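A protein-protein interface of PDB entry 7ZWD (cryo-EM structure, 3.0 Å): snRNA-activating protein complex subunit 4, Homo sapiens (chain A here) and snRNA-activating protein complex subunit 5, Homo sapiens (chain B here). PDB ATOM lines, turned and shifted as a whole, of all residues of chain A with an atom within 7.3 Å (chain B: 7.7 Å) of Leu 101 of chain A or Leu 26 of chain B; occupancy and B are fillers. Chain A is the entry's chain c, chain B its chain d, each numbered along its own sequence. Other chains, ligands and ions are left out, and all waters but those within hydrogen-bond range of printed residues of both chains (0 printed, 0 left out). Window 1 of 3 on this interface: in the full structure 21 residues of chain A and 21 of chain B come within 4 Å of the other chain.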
ATOM      1  N   TYR A  93       9.686 -14.799 -28.904  1.00  0.00           N
ATOM      2  CA  TYR A  93      10.613 -14.676 -27.780  1.00  0.00           C
ATOM      3  C   TYR A  93      11.872 -13.906 -28.175  1.00  0.00           C
ATOM      4  O   TYR A  93      12.352 -13.064 -27.401  1.00  0.00           O
ATOM      5  CB  TYR A  93      10.962 -16.058 -27.225  1.00  0.00           C
ATOM      6  CG  TYR A  93      11.871 -16.024 -26.014  1.00  0.00           C
ATOM      7  CD1 TYR A  93      11.469 -15.404 -24.837  1.00  0.00           C
ATOM      8  CD2 TYR A  93      13.114 -16.639 -26.036  1.00  0.00           C
ATOM      9  CE1 TYR A  93      12.290 -15.376 -23.727  1.00  0.00           C
ATOM     10  CE2 TYR A  93      13.943 -16.617 -24.930  1.00  0.00           C
ATOM     11  CZ  TYR A  93      13.526 -15.986 -23.778  1.00  0.00           C
ATOM     12  OH  TYR A  93      14.347 -15.963 -22.674  1.00  0.00           O
ATOM     13  N   GLN A  94      12.413 -14.166 -29.370  1.00  0.00           N
ATOM     14  CA  GLN A  94      13.476 -13.320 -29.902  1.00  0.00           C
ATOM     15  C   GLN A  94      13.024 -11.872 -30.006  1.00  0.00           C
ATOM     16  O   GLN A  94      13.813 -10.957 -29.763  1.00  0.00           O
ATOM     17  CB  GLN A  94      13.974 -13.842 -31.254  1.00  0.00           C
ATOM     18  CG  GLN A  94      14.480 -15.271 -31.266  1.00  0.00           C
ATOM     19  CD  GLN A  94      15.548 -15.492 -32.323  1.00  0.00           C
ATOM     20  OE1 GLN A  94      16.548 -16.166 -32.076  1.00  0.00           O
ATOM     21  NE2 GLN A  94      15.344 -14.919 -33.501  1.00  0.00           N
ATOM     22  N   GLU A  95      11.756 -11.644 -30.346  1.00  0.00           N
ATOM     23  CA  GLU A  95      11.259 -10.281 -30.495  1.00  0.00           C
ATOM     24  C   GLU A  95      11.245  -9.552 -29.156  1.00  0.00           C
ATOM     25  O   GLU A  95      11.673  -8.393 -29.066  1.00  0.00           O
ATOM     26  CB  GLU A  95       9.864 -10.306 -31.129  1.00  0.00           C
ATOM     27  CG  GLU A  95       9.134  -8.962 -31.202  1.00  0.00           C
ATOM     28  CD  GLU A  95       8.432  -8.585 -29.910  1.00  0.00           C
ATOM     29  OE1 GLU A  95       8.636  -7.452 -29.427  1.00  0.00           O
ATOM     30  OE2 GLU A  95       7.674  -9.424 -29.380  1.00  0.00           O
ATOM     31  N   VAL A  96      10.763 -10.212 -28.102  1.00  0.00           N
ATOM     32  CA  VAL A  96      10.695  -9.544 -26.803  1.00  0.00           C
ATOM     33  C   VAL A  96      12.099  -9.343 -26.233  1.00  0.00           C
ATOM     34  O   VAL A  96      12.413  -8.285 -25.671  1.00  0.00           O
ATOM     35  CB  VAL A  96       9.776 -10.312 -25.831  1.00  0.00           C
ATOM     36  CG1 VAL A  96      10.214 -11.751 -25.663  1.00  0.00           C
ATOM     37  CG2 VAL A  96       9.719  -9.604 -24.480  1.00  0.00           C
ATOM     38  N   ILE A  97      12.984 -10.331 -26.409  1.00  0.00           N
ATOM     39  CA  ILE A  97      14.340 -10.134 -25.899  1.00  0.00           C
ATOM     40  C   ILE A  97      15.093  -9.122 -26.759  1.00  0.00           C
ATOM     41  O   ILE A  97      16.020  -8.463 -26.280  1.00  0.00           O
ATOM     42  CB  ILE A  97      15.101 -11.469 -25.792  1.00  0.00           C
ATOM     43  CG1 ILE A  97      16.458 -11.246 -25.122  1.00  0.00           C
ATOM     44  CG2 ILE A  97      15.327 -12.067 -27.159  1.00  0.00           C
ATOM     45  CD1 ILE A  97      17.218 -12.507 -24.843  1.00  0.00           C
ATOM     46  N   GLN A  98      14.689  -8.941 -28.018  1.00  0.00           N
ATOM     47  CA  GLN A  98      15.321  -7.933 -28.862  1.00  0.00           C
ATOM     48  C   GLN A  98      14.854  -6.536 -28.482  1.00  0.00           C
ATOM     49  O   GLN A  98      15.636  -5.582 -28.519  1.00  0.00           O
ATOM     50  CB  GLN A  98      15.022  -8.225 -30.334  1.00  0.00           C
ATOM     51  CG  GLN A  98      15.554  -7.198 -31.332  1.00  0.00           C
ATOM     52  CD  GLN A  98      16.952  -6.699 -31.002  1.00  0.00           C
ATOM     53  OE1 GLN A  98      17.837  -7.478 -30.647  1.00  0.00           O
ATOM     54  NE2 GLN A  98      17.154  -5.391 -31.116  1.00  0.00           N
ATOM     55  N   GLU A  99      13.576  -6.394 -28.120  1.00  0.00           N
ATOM     56  CA  GLU A  99      13.124  -5.142 -27.523  1.00  0.00           C
ATOM     57  C   GLU A  99      13.910  -4.848 -26.250  1.00  0.00           C
ATOM     58  O   GLU A  99      14.340  -3.709 -26.019  1.00  0.00           O
ATOM     59  CB  GLU A  99      11.620  -5.209 -27.239  1.00  0.00           C
ATOM     60  CG  GLU A  99      10.935  -3.866 -26.948  1.00  0.00           C
ATOM     61  CD  GLU A  99      11.348  -3.245 -25.624  1.00  0.00           C
ATOM     62  OE1 GLU A  99      11.297  -3.948 -24.594  1.00  0.00           O
ATOM     63  OE2 GLU A  99      11.726  -2.055 -25.615  1.00  0.00           O
ATOM     64  N   LYS A 100      14.114  -5.872 -25.417  1.00  0.00           N
ATOM     65  CA  LYS A 100      14.901  -5.691 -24.201  1.00  0.00           C
ATOM     66  C   LYS A 100      16.332  -5.269 -24.520  1.00  0.00           C
ATOM     67  O   LYS A 100      16.888  -4.388 -23.855  1.00  0.00           O
ATOM     68  CB  LYS A 100      14.894  -6.980 -23.381  1.00  0.00           C
ATOM     69  CG  LYS A 100      15.093  -6.755 -21.900  1.00  0.00           C
ATOM     70  CD  LYS A 100      13.758  -6.609 -21.199  1.00  0.00           C
ATOM     71  CE  LYS A 100      13.937  -6.079 -19.797  1.00  0.00           C
ATOM     72  NZ  LYS A 100      14.630  -7.055 -18.917  1.00  0.00           N
ATOM     73  N   LEU A 101      16.938  -5.888 -25.535  1.00  0.00           N
ATOM     74  CA  LEU A 101      18.296  -5.533 -25.934  1.00  0.00           C
ATOM     75  C   LEU A 101      18.369  -4.113 -26.471  1.00  0.00           C
ATOM     76  O   LEU A 101      19.331  -3.393 -26.198  1.00  0.00           O
ATOM     77  CB  LEU A 101      18.816  -6.520 -26.976  1.00  0.00           C
ATOM     78  CG  LEU A 101      19.233  -7.894 -26.464  1.00  0.00           C
ATOM     79  CD1 LEU A 101      19.497  -8.828 -27.619  1.00  0.00           C
ATOM     80  CD2 LEU A 101      20.487  -7.729 -25.621  1.00  0.00           C
ATOM     81  N   ALA A 102      17.374  -3.697 -27.253  1.00  0.00           N
ATOM     82  CA  ALA A 102      17.365  -2.327 -27.750  1.00  0.00           C
ATOM     83  C   ALA A 102      17.262  -1.337 -26.599  1.00  0.00           C
ATOM     84  O   ALA A 102      17.994  -0.341 -26.563  1.00  0.00           O
ATOM     85  CB  ALA A 102      16.216  -2.128 -28.737  1.00  0.00           C
ATOM     86  N   GLU A 103      16.378  -1.608 -25.638  1.00  0.00           N
ATOM     87  CA  GLU A 103      16.254  -0.726 -24.482  1.00  0.00           C
ATOM     88  C   GLU A 103      17.558  -0.675 -23.692  1.00  0.00           C
ATOM     89  O   GLU A 103      18.010   0.404 -23.286  1.00  0.00           O
ATOM     90  CB  GLU A 103      15.086  -1.191 -23.606  1.00  0.00           C
ATOM     91  CG  GLU A 103      14.725  -0.281 -22.433  1.00  0.00           C
ATOM     92  CD  GLU A 103      15.585  -0.497 -21.206  1.00  0.00           C
ATOM     93  OE1 GLU A 103      16.341  -1.489 -21.166  1.00  0.00           O
ATOM     94  OE2 GLU A 103      15.490   0.324 -20.271  1.00  0.00           O
ATOM     95  N   ALA A 104      18.190  -1.833 -23.484  1.00  0.00           N
ATOM     96  CA  ALA A 104      19.422  -1.878 -22.705  1.00  0.00           C
ATOM     97  C   ALA A 104      20.562  -1.170 -23.429  1.00  0.00           C
ATOM     98  O   ALA A 104      21.348  -0.449 -22.807  1.00  0.00           O
ATOM     99  CB  ALA A 104      19.790  -3.329 -22.401  1.00  0.00           C
ATOM    100  N   ASN A 105      20.665  -1.357 -24.747  1.00  0.00           N
ATOM    101  CA  ASN A 105      21.701  -0.677 -25.515  1.00  0.00           C
ATOM    102  C   ASN A 105      21.455   0.825 -25.563  1.00  0.00           C
ATOM    103  O   ASN A 105      22.406   1.610 -25.623  1.00  0.00           O
ATOM    104  CB  ASN A 105      21.779  -1.259 -26.926  1.00  0.00           C
ATOM    105  CG  ASN A 105      22.343  -2.670 -26.947  1.00  0.00           C
ATOM    106  OD1 ASN A 105      22.095  -3.466 -26.043  1.00  0.00           O
ATOM    107  ND2 ASN A 105      23.108  -2.984 -27.987  1.00  0.00           N
ATOM    108  N   LEU A 106      20.190   1.252 -25.527  1.00  0.00           N
ATOM    109  CA  LEU A 106      19.912   2.683 -25.438  1.00  0.00           C
ATOM    110  C   LEU A 106      20.317   3.243 -24.081  1.00  0.00           C
ATOM    111  O   LEU A 106      20.845   4.358 -23.996  1.00  0.00           O
ATOM    112  CB  LEU A 106      18.437   2.963 -25.726  1.00  0.00           C
ATOM    113  CG  LEU A 106      18.079   3.328 -27.171  1.00  0.00           C
ATOM    114  CD1 LEU A 106      18.697   4.670 -27.520  1.00  0.00           C
ATOM    115  CD2 LEU A 106      18.539   2.273 -28.161  1.00  0.00           C
ATOM    116  N   LEU A 107      20.082   2.489 -23.002  1.00  0.00           N
ATOM    117  CA  LEU A 107      20.613   2.918 -21.709  1.00  0.00           C
ATOM    118  C   LEU A 107      22.135   2.971 -21.734  1.00  0.00           C
ATOM    119  O   LEU A 107      22.738   3.860 -21.125  1.00  0.00           O
ATOM    120  CB  LEU A 107      20.142   2.003 -20.583  1.00  0.00           C
ATOM    121  CG  LEU A 107      18.685   1.571 -20.521  1.00  0.00           C
ATOM    122  CD1 LEU A 107      18.530   0.571 -19.404  1.00  0.00           C
ATOM    123  CD2 LEU A 107      17.779   2.769 -20.302  1.00  0.00           C
ATOM    124  N   LEU B  18      24.099  -7.555 -17.818  1.00  0.00           N
ATOM    125  CA  LEU B  18      22.792  -7.942 -18.347  1.00  0.00           C
ATOM    126  C   LEU B  18      22.830  -8.102 -19.862  1.00  0.00           C
ATOM    127  O   LEU B  18      22.222  -9.030 -20.409  1.00  0.00           O
ATOM    128  CB  LEU B  18      21.723  -6.925 -17.948  1.00  0.00           C
ATOM    129  CG  LEU B  18      21.665  -6.476 -16.491  1.00  0.00           C
ATOM    130  CD1 LEU B  18      20.525  -5.502 -16.287  1.00  0.00           C
ATOM    131  CD2 LEU B  18      21.490  -7.685 -15.595  1.00  0.00           C
ATOM    132  N   LYS B  19      23.530  -7.205 -20.559  1.00  0.00           N
ATOM    133  CA  LYS B  19      23.630  -7.324 -22.010  1.00  0.00           C
ATOM    134  C   LYS B  19      24.401  -8.568 -22.410  1.00  0.00           C
ATOM    135  O   LYS B  19      24.065  -9.210 -23.405  1.00  0.00           O
ATOM    136  CB  LYS B  19      24.286  -6.085 -22.613  1.00  0.00           C
ATOM    137  CG  LYS B  19      23.532  -4.813 -22.359  1.00  0.00           C
ATOM    138  CD  LYS B  19      24.073  -3.692 -23.204  1.00  0.00           C
ATOM    139  CE  LYS B  19      23.813  -2.373 -22.530  1.00  0.00           C
ATOM    140  NZ  LYS B  19      22.745  -2.457 -21.499  1.00  0.00           N
ATOM    141  N   ALA B  20      25.438  -8.926 -21.652  1.00  0.00           N
ATOM    142  CA  ALA B  20      26.161 -10.162 -21.931  1.00  0.00           C
ATOM    143  C   ALA B  20      25.243 -11.367 -21.795  1.00  0.00           C
ATOM    144  O   ALA B  20      25.214 -12.247 -22.666  1.00  0.00           O
ATOM    145  CB  ALA B  20      27.364 -10.289 -20.998  1.00  0.00           C
ATOM    146  N   ALA B  21      24.475 -11.420 -20.702  1.00  0.00           N
ATOM    147  CA  ALA B  21      23.544 -12.530 -20.513  1.00  0.00           C
ATOM    148  C   ALA B  21      22.519 -12.594 -21.643  1.00  0.00           C
ATOM    149  O   ALA B  21      22.280 -13.666 -22.222  1.00  0.00           O
ATOM    150  CB  ALA B  21      22.844 -12.403 -19.161  1.00  0.00           C
ATOM    151  N   LEU B  22      21.912 -11.453 -21.979  1.00  0.00           N
ATOM    152  CA  LEU B  22      20.888 -11.437 -23.019  1.00  0.00           C
ATOM    153  C   LEU B  22      21.475 -11.743 -24.392  1.00  0.00           C
ATOM    154  O   LEU B  22      20.801 -12.334 -25.238  1.00  0.00           O
ATOM    155  CB  LEU B  22      20.170 -10.086 -23.028  1.00  0.00           C
ATOM    156  CG  LEU B  22      18.890  -9.975 -22.197  1.00  0.00           C
ATOM    157  CD1 LEU B  22      19.190  -9.927 -20.710  1.00  0.00           C
ATOM    158  CD2 LEU B  22      18.088  -8.755 -22.628  1.00  0.00           C
ATOM    159  N   HIS B  23      22.731 -11.361 -24.632  1.00  0.00           N
ATOM    160  CA  HIS B  23      23.363 -11.662 -25.910  1.00  0.00           C
ATOM    161  C   HIS B  23      23.676 -13.146 -26.036  1.00  0.00           C
ATOM    162  O   HIS B  23      23.516 -13.724 -27.115  1.00  0.00           O
ATOM    163  CB  HIS B  23      24.631 -10.829 -26.088  1.00  0.00           C
ATOM    164  CG  HIS B  23      24.371  -9.374 -26.326  1.00  0.00           C
ATOM    165  ND1 HIS B  23      25.098  -8.378 -25.709  1.00  0.00           N
ATOM    166  CD2 HIS B  23      23.464  -8.747 -27.111  1.00  0.00           C
ATOM    167  CE1 HIS B  23      24.651  -7.200 -26.107  1.00  0.00           C
ATOM    168  NE2 HIS B  23      23.658  -7.396 -26.957  1.00  0.00           N
ATOM    169  N   ASP B  24      24.135 -13.777 -24.953  1.00  0.00           N
ATOM    170  CA  ASP B  24      24.288 -15.229 -24.977  1.00  0.00           C
ATOM    171  C   ASP B  24      22.947 -15.906 -25.233  1.00  0.00           C
ATOM    172  O   ASP B  24      22.858 -16.876 -26.001  1.00  0.00           O
ATOM    173  CB  ASP B  24      24.902 -15.725 -23.667  1.00  0.00           C
ATOM    174  CG  ASP B  24      26.149 -14.957 -23.281  1.00  0.00           C
ATOM    175  OD1 ASP B  24      26.882 -14.513 -24.189  1.00  0.00           O
ATOM    176  OD2 ASP B  24      26.398 -14.798 -22.067  1.00  0.00           O
ATOM    177  N   GLN B  25      21.887 -15.401 -24.592  1.00  0.00           N
ATOM    178  CA  GLN B  25      20.551 -15.937 -24.835  1.00  0.00           C
ATOM    179  C   GLN B  25      20.155 -15.784 -26.300  1.00  0.00           C
ATOM    180  O   GLN B  25      19.612 -16.714 -26.901  1.00  0.00           O
ATOM    181  CB  GLN B  25      19.539 -15.243 -23.920  1.00  0.00           C
ATOM    182  CG  GLN B  25      18.100 -15.780 -23.957  1.00  0.00           C
ATOM    183  CD  GLN B  25      17.995 -17.294 -23.862  1.00  0.00           C
ATOM    184  OE1 GLN B  25      18.270 -18.014 -24.820  1.00  0.00           O
ATOM    185  NE2 GLN B  25      17.586 -17.782 -22.697  1.00  0.00           N
ATOM    186  N   LEU B  26      20.450 -14.627 -26.900  1.00  0.00           N
ATOM    187  CA  LEU B  26      20.123 -14.408 -28.307  1.00  0.00           C
ATOM    188  C   LEU B  26      20.903 -15.346 -29.220  1.00  0.00           C
ATOM    189  O   LEU B  26      20.346 -15.891 -30.182  1.00  0.00           O
ATOM    190  CB  LEU B  26      20.398 -12.956 -28.699  1.00  0.00           C
ATOM    191  CG  LEU B  26      19.562 -12.432 -29.870  1.00  0.00           C
ATOM    192  CD1 LEU B  26      18.089 -12.353 -29.502  1.00  0.00           C
ATOM    193  CD2 LEU B  26      20.083 -11.090 -30.365  1.00  0.00           C
ATOM    194  N   ASN B  27      22.200 -15.521 -28.958  1.00  0.00           N
ATOM    195  CA  ASN B  27      23.004 -16.398 -29.803  1.00  0.00           C
ATOM    196  C   ASN B  27      22.511 -17.837 -29.730  1.00  0.00           C
ATOM    197  O   ASN B  27      22.317 -18.484 -30.768  1.00  0.00           O
ATOM    198  CB  ASN B  27      24.481 -16.313 -29.416  1.00  0.00           C
ATOM    199  CG  ASN B  27      24.983 -14.885 -29.340  1.00  0.00           C
ATOM    200  OD1 ASN B  27      24.418 -13.981 -29.956  1.00  0.00           O
ATOM    201  ND2 ASN B  27      26.051 -14.674 -28.579  1.00  0.00           N
ATOM    202  N   ARG B  28      22.286 -18.353 -28.518  1.00  0.00           N
ATOM    203  CA  ARG B  28      21.764 -19.710 -28.410  1.00  0.00           C
ATOM    204  C   ARG B  28      20.367 -19.807 -29.015  1.00  0.00           C
ATOM    205  O   ARG B  28      20.009 -20.833 -29.602  1.00  0.00           O
ATOM    206  CB  ARG B  28      21.775 -20.178 -26.952  1.00  0.00           C
ATOM    207  CG  ARG B  28      20.815 -19.460 -26.027  1.00  0.00           C
ATOM    208  CD  ARG B  28      20.544 -20.280 -24.770  1.00  0.00           C
ATOM    209  NE  ARG B  28      21.767 -20.722 -24.100  1.00  0.00           N
ATOM    210  CZ  ARG B  28      22.655 -19.916 -23.523  1.00  0.00           C
ATOM    211  NH1 ARG B  28      22.472 -18.602 -23.511  1.00  0.00           N
ATOM    212  NH2 ARG B  28      23.731 -20.430 -22.942  1.00  0.00           N
ATOM    213  N   LEU B  29      19.584 -18.726 -28.935  1.00  0.00           N
ATOM    214  CA  LEU B  29      18.266 -18.711 -29.559  1.00  0.00           C
ATOM    215  C   LEU B  29      18.365 -18.871 -31.068  1.00  0.00           C
ATOM    216  O   LEU B  29      17.646 -19.681 -31.659  1.00  0.00           O
ATOM    217  CB  LEU B  29      17.542 -17.410 -29.218  1.00  0.00           C
ATOM    218  CG  LEU B  29      16.653 -17.356 -27.978  1.00  0.00           C
ATOM    219  CD1 LEU B  29      15.836 -16.078 -28.013  1.00  0.00           C
ATOM    220  CD2 LEU B  29      15.752 -18.577 -27.903  1.00  0.00           C
ATOM    221  N   LYS B  30      19.245 -18.102 -31.711  1.00  0.00           N
ATOM    222  CA  LYS B  30      19.375 -18.208 -33.161  1.00  0.00           C
ATOM    223  C   LYS B  30      19.969 -19.551 -33.566  1.00  0.00           C
ATOM    224  O   LYS B  30      19.662 -20.072 -34.646  1.00  0.00           O
ATOM    225  CB  LYS B  30      20.210 -17.056 -33.723  1.00  0.00           C
ATOM    226  CG  LYS B  30      19.758 -15.669 -33.291  1.00  0.00           C
ATOM    227  CD  LYS B  30      20.779 -14.608 -33.674  1.00  0.00           C
ATOM    228  CE  LYS B  30      21.816 -14.396 -32.585  1.00  0.00           C
ATOM    229  NZ  LYS B  30      22.456 -13.054 -32.685  1.00  0.00           N
ATOM    230  N   VAL B  31      20.811 -20.137 -32.712  1.00  0.00           N
ATOM    231  CA  VAL B  31      21.291 -21.488 -32.998  1.00  0.00           C
ATOM    232  C   VAL B  31      20.132 -22.479 -32.970  1.00  0.00           C
ATOM    233  O   VAL B  31      20.021 -23.356 -33.839  1.00  0.00           O
ATOM    234  CB  VAL B  31      22.410 -21.885 -32.019  1.00  0.00           C
ATOM    235  CG1 VAL B  31      22.816 -23.333 -32.242  1.00  0.00           C
ATOM    236  CG2 VAL B  31      23.611 -20.973 -32.193  1.00  0.00           C
ATOM    237  N   GLU B  32      19.242 -22.351 -31.979  1.00  0.00           N
ATOM    238  CA  GLU B  32      18.029 -23.164 -31.974  1.00  0.00           C
ATOM    239  C   GLU B  32      17.191 -22.914 -33.221  1.00  0.00           C
ATOM    240  O   GLU B  32      16.590 -23.839 -33.768  1.00  0.00           O
ATOM    241  CB  GLU B  32      17.193 -22.902 -30.716  1.00  0.00           C
ATOM    242  CG  GLU B  32      17.949 -22.949 -29.404  1.00  0.00           C
ATOM    243  CD  GLU B  32      17.160 -22.337 -28.260  1.00  0.00           C
ATOM    244  OE1 GLU B  32      17.787 -21.804 -27.320  1.00  0.00           O
ATOM    245  OE2 GLU B  32      15.913 -22.385 -28.304  1.00  0.00           O
ATOM    246  N   GLU B  33      17.131 -21.660 -33.676  1.00  0.00           N
ATOM    247  CA  GLU B  33      16.373 -21.350 -34.888  1.00  0.00           C
ATOM    248  C   GLU B  33      16.933 -22.086 -36.098  1.00  0.00           C
ATOM    249  O   GLU B  33      16.177 -22.669 -36.884  1.00  0.00           O
ATOM    250  CB  GLU B  33      16.356 -19.841 -35.145  1.00  0.00           C
ATOM    251  CG  GLU B  33      15.830 -18.997 -33.997  1.00  0.00           C
ATOM    252  CD  GLU B  33      14.313 -18.969 -33.918  1.00  0.00           C
ATOM    253  OE1 GLU B  33      13.664 -20.004 -34.175  1.00  0.00           O
ATOM    254  OE2 GLU B  33      13.765 -17.900 -33.580  1.00  0.00           O
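Among the printed residues, pairs that only touch across the chains: Gln 94 of chain A with Leu 29 of chain B (3.3 Å), Tyr 93 of chain A with Leu 29 of chain B (3.4 Å), Leu 101 of chain A with His 23 of chain B (3.5 Å), Asn 105 of chain A with Lys 19 of chain B (3.5 Å), Ile 97 of chain A with Gln 25 of chain B (3.5 Å), Leu 101 of chain A with Leu 22 of chain B (3.5 Å), Leu 101 of chain A with Leu 26 of chain B (3.6 Å), Ile 97 of chain A with Leu 22 of chain B (3.6 Å), Ile 97 of chain A with Leu 26 of chain B (3.6 Å), Lys 100 of chain A with Leu 22 of chain B (3.7 Å) and Tyr 93 of chain A with Gln 25 of chain B (3.7 Å).
The side-chain carboxylate of Glu 33 of chain B sits close to the side-chain amide nitrogen of Gln 94 of chain A, at 3.4 Å. The backbone carbonyl oxygen (O) of Ala 104 of chain A lies within hydrogen-bond range of the side-chain amino group (NZ) of Lys 19 of chain B (2.8 Å). The side-chain amide oxygen (OE1) of Gln 94 of chain A is in hydrogen-bond range of the backbone NH (N) of Lys 30 of chain B (3.3 Å).
Printed residues of chain B that touch a printed residue of chain A: Lys 19, Leu 22, His 23, Gln 25, Leu 26, Leu 29, Lys 30 and Glu 33. Printed residues of chain A that touch a printed residue of chain B: Tyr 93, Gln 94, Ile 97, Lys 100, Leu 101, Ala 104 and Asn 105. Among the printed residues, no Asp or Glu carboxylate lies within 4 Å of a Lys or Arg side-chain nitrogen of the other chain.
Of the printed residues of chain B, Lys 100 of chain A touches Leu 22 (3.7 Å). Of chain B, only Leu 22, His 23 and Leu 26 come within 4 Å of Leu 101 of chain A. Leu 26 of chain B touches two residues of chain A. Printed residues of chain A within 4 Å of Leu 29 of chain B: Tyr 93 and Gln 94. Printed residues of chain A within 4 Å of Lys 30 of chain B: Gln 94 (3.3 Å). Printed residues of chain A within 4 Å of Glu 33 of chain B: Gln 94.
The side-chain amide oxygen (OD1) of Asn 105 of chain A lies close to the backbone carbonyl oxygen (O) of Leu 101 of chain A (2.8 Å). The backbone carbonyl oxygen (O) of His 23 of chain B lies close to the side-chain amide oxygen (OD1) of Asn 27 of chain B (3.0 Å). The side-chain amide oxygen (OD1) of Asn 27 of chain B sits at hydrogen-bond distance from the side-chain amino group (NZ) of Lys 30 of chain B (3.5 Å). The backbone carbonyl oxygen of Lys 19 of chain B lies within hydrogen-bond range of a ring nitrogen (ND1) of His 23 of chain B (2.7 Å).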
